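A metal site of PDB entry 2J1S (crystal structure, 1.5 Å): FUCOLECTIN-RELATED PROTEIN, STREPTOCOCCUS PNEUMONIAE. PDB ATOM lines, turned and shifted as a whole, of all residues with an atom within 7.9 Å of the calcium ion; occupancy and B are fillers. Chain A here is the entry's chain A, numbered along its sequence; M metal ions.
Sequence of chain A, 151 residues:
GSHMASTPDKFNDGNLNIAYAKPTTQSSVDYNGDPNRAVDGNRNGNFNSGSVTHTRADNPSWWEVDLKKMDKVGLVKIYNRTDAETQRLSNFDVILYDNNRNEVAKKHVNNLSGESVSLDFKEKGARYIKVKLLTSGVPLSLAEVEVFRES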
ATOM      1  N   PRO A  35      10.902 -22.745 -22.150  1.00  0.00           N
ATOM      2  CA  PRO A  35      11.725 -23.959 -22.218  1.00  0.00           C
ATOM      3  C   PRO A  35      13.146 -23.723 -22.588  1.00  0.00           C
ATOM      4  O   PRO A  35      14.024 -24.562 -22.267  1.00  0.00           O
ATOM      5  CB  PRO A  35      11.039 -24.814 -23.263  1.00  0.00           C
ATOM      6  CG  PRO A  35      10.201 -23.830 -24.035  1.00  0.00           C
ATOM      7  CD  PRO A  35       9.793 -22.782 -23.106  1.00  0.00           C
ATOM      8  N   ASN A  36      13.443 -22.573 -23.203  1.00  0.00           N
ATOM      9  CA  ASN A  36      14.810 -22.278 -23.581  1.00  0.00           C
ATOM     10  C   ASN A  36      15.704 -22.001 -22.363  1.00  0.00           C
ATOM     11  O   ASN A  36      16.921 -21.990 -22.482  1.00  0.00           O
ATOM     12  CB  ASN A  36      14.871 -21.163 -24.607  1.00  0.00           C
ATOM     13  CG  ASN A  36      14.509 -19.775 -24.094  1.00  0.00           C
ATOM     14  OD1 ASN A  36      14.941 -18.751 -24.724  1.00  0.00           O
ATOM     15  ND2 ASN A  36      13.712 -19.686 -23.072  1.00  0.00           N
ATOM     16  N   ARG A  37      15.102 -21.844 -21.202  1.00  0.00           N
ATOM     17  CA  ARG A  37      15.903 -21.643 -20.000  1.00  0.00           C
ATOM     18  C   ARG A  37      16.741 -22.854 -19.628  1.00  0.00           C
ATOM     19  O   ARG A  37      17.754 -22.698 -18.941  1.00  0.00           O
ATOM     20  CB  ARG A  37      14.983 -21.159 -18.871  1.00  0.00           C
ATOM     21  CG  ARG A  37      14.367 -19.783 -19.160  1.00  0.00           C
ATOM     22  CD  ARG A  37      13.516 -19.211 -18.034  1.00  0.00           C
ATOM     23  NE  ARG A  37      12.951 -17.966 -18.529  1.00  0.00           N
ATOM     24  CZ  ARG A  37      12.424 -16.986 -17.807  1.00  0.00           C
ATOM     25  NH1 ARG A  37      11.999 -15.897 -18.474  1.00  0.00           N
ATOM     26  NH2 ARG A  37      12.286 -17.076 -16.485  1.00  0.00           N
ATOM     27  N   ALA A  38      16.334 -24.063 -20.083  1.00  0.00           N
ATOM     28  CA  ALA A  38      17.105 -25.285 -19.768  1.00  0.00           C
ATOM     29  C   ALA A  38      18.246 -25.510 -20.746  1.00  0.00           C
ATOM     30  O   ALA A  38      19.018 -26.435 -20.593  1.00  0.00           O
ATOM     31  CB  ALA A  38      16.206 -26.554 -19.654  1.00  0.00           C
ATOM     32  N   VAL A  39      18.397 -24.625 -21.738  1.00  0.00           N
ATOM     33  CA  VAL A  39      19.578 -24.698 -22.641  1.00  0.00           C
ATOM     34  C   VAL A  39      20.299 -23.340 -22.773  1.00  0.00           C
ATOM     35  O   VAL A  39      20.925 -23.059 -23.777  1.00  0.00           O
ATOM     36  CB  VAL A  39      19.226 -25.278 -24.036  1.00  0.00           C
ATOM     37  CG1 VAL A  39      18.686 -26.711 -23.905  1.00  0.00           C
ATOM     38  CG2 VAL A  39      18.212 -24.414 -24.813  1.00  0.00           C
ATOM     39  N   ASP A  40      20.206 -22.523 -21.722  1.00  0.00           N
ATOM     40  CA  ASP A  40      20.771 -21.160 -21.744  1.00  0.00           C
ATOM     41  C   ASP A  40      22.224 -21.095 -21.240  1.00  0.00           C
ATOM     42  O   ASP A  40      22.833 -20.017 -21.230  1.00  0.00           O
ATOM     43  CB  ASP A  40      19.843 -20.177 -21.037  1.00  0.00           C
ATOM     44  CG  ASP A  40      19.793 -20.355 -19.526  1.00  0.00           C
ATOM     45  OD1 ASP A  40      20.402 -21.288 -18.978  1.00  0.00           O
ATOM     46  OD2 ASP A  40      19.140 -19.577 -18.805  1.00  0.00           O
ATOM     47  N   GLY A  41      22.808 -22.262 -20.956  1.00  0.00           N
ATOM     48  CA  GLY A  41      24.189 -22.361 -20.514  1.00  0.00           C
ATOM     49  C   GLY A  41      24.379 -22.133 -19.022  1.00  0.00           C
ATOM     50  O   GLY A  41      25.537 -22.177 -18.544  1.00  0.00           O
ATOM     51  N   ASN A  42      23.287 -21.899 -18.304  1.00  0.00           N
ATOM     52  CA  ASN A  42      23.321 -21.554 -16.891  1.00  0.00           C
ATOM     53  C   ASN A  42      22.704 -22.688 -16.041  1.00  0.00           C
ATOM     54  O   ASN A  42      21.509 -23.028 -16.176  1.00  0.00           O
ATOM     55  CB  ASN A  42      22.609 -20.226 -16.680  1.00  0.00           C
ATOM     56  CG  ASN A  42      22.725 -19.722 -15.258  1.00  0.00           C
ATOM     57  OD1 ASN A  42      23.425 -20.303 -14.428  1.00  0.00           O
ATOM     58  ND2 ASN A  42      22.027 -18.609 -14.963  1.00  0.00           N
ATOM     59  N   ARG A  43      23.538 -23.243 -15.149  1.00  0.00           N
ATOM     60  CA  ARG A  43      23.100 -24.331 -14.307  1.00  0.00           C
ATOM     61  C   ARG A  43      22.357 -23.846 -13.044  1.00  0.00           C
ATOM     62  O   ARG A  43      21.788 -24.654 -12.282  1.00  0.00           O
ATOM     63  CB  ARG A  43      24.318 -25.158 -13.916  1.00  0.00           C
ATOM     64  CG  ARG A  43      24.953 -25.883 -15.029  1.00  0.00           C
ATOM     65  CD  ARG A  43      26.222 -26.582 -14.581  1.00  0.00           C
ATOM     66  NE  ARG A  43      26.830 -27.312 -15.658  1.00  0.00           N
ATOM     67  CZ  ARG A  43      27.979 -27.984 -15.573  1.00  0.00           C
ATOM     68  NH1 ARG A  43      28.462 -28.625 -16.649  1.00  0.00           N
ATOM     69  NH2 ARG A  43      28.657 -28.012 -14.419  1.00  0.00           N
ATOM     70  N   ASN A  44      22.369 -22.545 -12.790  1.00  0.00           N
ATOM     71  CA  ASN A  44      21.690 -21.987 -11.611  1.00  0.00           C
ATOM     72  C   ASN A  44      20.254 -22.552 -11.529  1.00  0.00           C
ATOM     73  O   ASN A  44      19.451 -22.431 -12.486  1.00  0.00           O
ATOM     74  CB  ASN A  44      21.705 -20.458 -11.682  1.00  0.00           C
ATOM     75  CG  ASN A  44      21.330 -19.755 -10.377  1.00  0.00           C
ATOM     76  OD1 ASN A  44      21.707 -18.528 -10.170  1.00  0.00           O
ATOM     77  ND2 ASN A  44      20.619 -20.425  -9.511  1.00  0.00           N
ATOM     78  N   GLY A  45      19.933 -23.159 -10.376  1.00  0.00           N
ATOM     79  CA  GLY A  45      18.646 -23.785 -10.133  1.00  0.00           C
ATOM     80  C   GLY A  45      17.668 -22.968  -9.302  1.00  0.00           C
ATOM     81  O   GLY A  45      16.580 -23.447  -8.993  1.00  0.00           O
ATOM     82  N   SER A  49      16.218 -16.697 -10.458  1.00  0.00           N
ATOM     83  CA  SER A  49      17.390 -16.303 -11.262  1.00  0.00           C
ATOM     84  C   SER A  49      17.099 -16.133 -12.748  1.00  0.00           C
ATOM     85  O   SER A  49      17.918 -15.552 -13.464  1.00  0.00           O
ATOM     86  CB  SER A  49      18.532 -17.373 -11.219  1.00  0.00           C
ATOM     87  OG  SER A  49      18.231 -18.616 -11.945  1.00  0.00           O
ATOM     88  N   GLY A  50      16.004 -16.726 -13.229  1.00  0.00           N
ATOM     89  CA  GLY A  50      15.709 -16.707 -14.635  1.00  0.00           C
ATOM     90  C   GLY A  50      16.250 -17.853 -15.445  1.00  0.00           C
ATOM     91  O   GLY A  50      16.020 -17.926 -16.661  1.00  0.00           O
ATOM     92  N   SER A  51      16.950 -18.762 -14.796  1.00  0.00           N
ATOM     93  CA  SER A  51      17.647 -19.875 -15.435  1.00  0.00           C
ATOM     94  C   SER A  51      16.848 -21.191 -15.565  1.00  0.00           C
ATOM     95  O   SER A  51      17.388 -22.150 -16.104  1.00  0.00           O
ATOM     96  CB  SER A  51      18.906 -20.217 -14.592  1.00  0.00           C
ATOM     97  OG  SER A  51      19.636 -21.395 -14.986  1.00  0.00           O
ATOM     98  N   VAL A  52      15.622 -21.217 -15.023  1.00  0.00           N
ATOM     99  CA  VAL A  52      14.860 -22.463 -14.733  1.00  0.00           C
ATOM    100  C   VAL A  52      13.507 -22.430 -15.461  1.00  0.00           C
ATOM    101  O   VAL A  52      12.771 -21.419 -15.449  1.00  0.00           O
ATOM    102  CB  VAL A  52      14.642 -22.644 -13.178  1.00  0.00           C
ATOM    103  CG1 VAL A  52      13.961 -23.963 -12.883  1.00  0.00           C
ATOM    104  CG2 VAL A  52      15.950 -22.598 -12.462  1.00  0.00           C
ATOM    105  N   THR A  53      13.170 -23.541 -16.132  1.00  0.00           N
ATOM    106  CA  THR A  53      11.885 -23.676 -16.794  1.00  0.00           C
ATOM    107  C   THR A  53      10.778 -23.944 -15.791  1.00  0.00           C
ATOM    108  O   THR A  53      11.023 -24.247 -14.614  1.00  0.00           O
ATOM    109  CB  THR A  53      11.915 -24.837 -17.832  1.00  0.00           C
ATOM    110  OG1 THR A  53      12.033 -26.100 -17.144  1.00  0.00           O
ATOM    111  CG2 THR A  53      13.141 -24.745 -18.786  1.00  0.00           C
ATOM    112  N   TYR A  79      19.839 -30.941 -14.619  1.00  0.00           N
ATOM    113  CA  TYR A  79      19.988 -30.138 -13.403  1.00  0.00           C
ATOM    114  C   TYR A  79      18.627 -29.681 -12.890  1.00  0.00           C
ATOM    115  O   TYR A  79      17.846 -29.059 -13.586  1.00  0.00           O
ATOM    116  CB  TYR A  79      20.893 -28.929 -13.672  1.00  0.00           C
ATOM    117  CG  TYR A  79      22.305 -29.322 -14.076  1.00  0.00           C
ATOM    118  CD1 TYR A  79      23.343 -29.338 -13.148  1.00  0.00           C
ATOM    119  CD2 TYR A  79      22.603 -29.710 -15.385  1.00  0.00           C
ATOM    120  CE1 TYR A  79      24.640 -29.683 -13.552  1.00  0.00           C
ATOM    121  CE2 TYR A  79      23.857 -30.087 -15.748  1.00  0.00           C
ATOM    122  CZ  TYR A  79      24.884 -30.060 -14.834  1.00  0.00           C
ATOM    123  OH  TYR A  79      26.179 -30.407 -15.201  1.00  0.00           O
ATOM    124  N   LEU A 142      13.187 -27.475 -14.855  1.00  0.00           N
ATOM    125  CA  LEU A 142      14.521 -27.903 -15.138  1.00  0.00           C
ATOM    126  C   LEU A 142      15.446 -26.683 -15.191  1.00  0.00           C
ATOM    127  O   LEU A 142      15.190 -25.710 -15.895  1.00  0.00           O
ATOM    128  CB  LEU A 142      14.612 -28.620 -16.495  1.00  0.00           C
ATOM    129  CG  LEU A 142      13.753 -29.871 -16.639  1.00  0.00           C
ATOM    130  CD1 LEU A 142      13.681 -30.243 -18.097  1.00  0.00           C
ATOM    131  CD2 LEU A 142      14.355 -31.007 -15.803  1.00  0.00           C
ATOM    132  N   ALA A 143      16.502 -26.758 -14.411  1.00  0.00           N
ATOM    133  CA  ALA A 143      17.492 -25.687 -14.407  1.00  0.00           C
ATOM    134  C   ALA A 143      18.348 -25.690 -15.683  1.00  0.00           C
ATOM    135  O   ALA A 143      18.714 -24.622 -16.222  1.00  0.00           O
ATOM    136  CB  ALA A 143      18.390 -25.786 -13.148  1.00  0.00           C
ATOM    137  N   GLU A 144      18.676 -26.900 -16.162  1.00  0.00           N
ATOM    138  CA  GLU A 144      19.511 -27.070 -17.323  1.00  0.00           C
ATOM    139  C   GLU A 144      19.545 -28.533 -17.724  1.00  0.00           C
ATOM    140  O   GLU A 144      19.476 -29.412 -16.886  1.00  0.00           O
ATOM    141  CB  GLU A 144      20.973 -26.543 -17.089  1.00  0.00           C
ATOM    142  CG  GLU A 144      21.790 -26.286 -18.359  1.00  0.00           C
ATOM    143  CD  GLU A 144      21.405 -25.047 -19.160  1.00  0.00           C
ATOM    144  OE1 GLU A 144      20.462 -24.289 -18.751  1.00  0.00           O
ATOM    145  OE2 GLU A 144      22.055 -24.858 -20.232  1.00  0.00           O
ATOM    146  N   VAL A 145      19.600 -28.737 -19.030  1.00  0.00           N
ATOM    147  CA  VAL A 145      19.806 -30.036 -19.634  1.00  0.00           C
ATOM    148  C   VAL A 145      20.950 -29.945 -20.584  1.00  0.00           C
ATOM    149  O   VAL A 145      20.894 -29.223 -21.567  1.00  0.00           O
ATOM    150  CB  VAL A 145      18.543 -30.598 -20.345  1.00  0.00           C
ATOM    151  CG1 VAL A 145      18.866 -31.990 -20.965  1.00  0.00           C
ATOM    152  CG2 VAL A 145      17.386 -30.675 -19.384  1.00  0.00           C
ATOM    153  N   GLU A 146      22.012 -30.660 -20.244  1.00  0.00           N
ATOM    154  CA  GLU A 146      23.196 -30.701 -21.061  1.00  0.00           C
ATOM    155  C   GLU A 146      23.316 -32.076 -21.739  1.00  0.00           C
ATOM    156  O   GLU A 146      23.066 -33.074 -21.107  1.00  0.00           O
ATOM    157  CB  GLU A 146      24.424 -30.380 -20.234  1.00  0.00           C
ATOM    158  CG  GLU A 146      24.367 -28.996 -19.586  1.00  0.00           C
ATOM    159  CD  GLU A 146      25.533 -28.661 -18.688  1.00  0.00           C
ATOM    160  OE1 GLU A 146      26.397 -29.551 -18.426  1.00  0.00           O
ATOM    161  OE2 GLU A 146      25.519 -27.507 -18.207  1.00  0.00           O
HETATM  162 CA    CA M   1      19.416 -22.750 -17.268  1.00  0.00          CA
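Within 4 Å of the calcium ion: Arg 37, Asp 40, Asn 42, Ser 51, Ala 143 and Glu 144.
The calcium ion is bound by O of Ala 143 (2.3 Å). O of Arg 37 is bound to the calcium ion, at 2.4 Å. The backbone carbonyl oxygen (O) of Asn 42 binds the calcium ion, 2.4 Å away. OE1 of Glu 144 binds the calcium ion, 2.4 Å away. The backbone carbonyl oxygen (O) of Ser 51 binds the calcium ion (2.4 Å). The calcium ion is bound by the side-chain carboxylate (OD1) of Asp 40, at 2.5 Å. The calcium ion is bound by the side-chain hydroxyl (OG) of Ser 51.
N of Tyr 79 is in hydrogen-bond range of O of Glu 144, at 2.8 Å. The side-chain carboxylate of Glu 144 sits at hydrogen-bond distance from the backbone NH of Gly 41 (2.8 Å). The backbone NH of Asn 44 lies within hydrogen-bond range of the side-chain amide oxygen of Asn 42, 3.0 Å away. N of Ser 51 is in hydrogen-bond range of OG of Ser 49, at 3.1 Å. The side-chain hydroxyl of Ser 51 sits close to the backbone carbonyl oxygen of Asn 44 (2.7 Å). The backbone carbonyl oxygen (O) of Tyr 79 sits at hydrogen-bond distance from the backbone NH (N) of Ala 143, 2.8 Å away.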
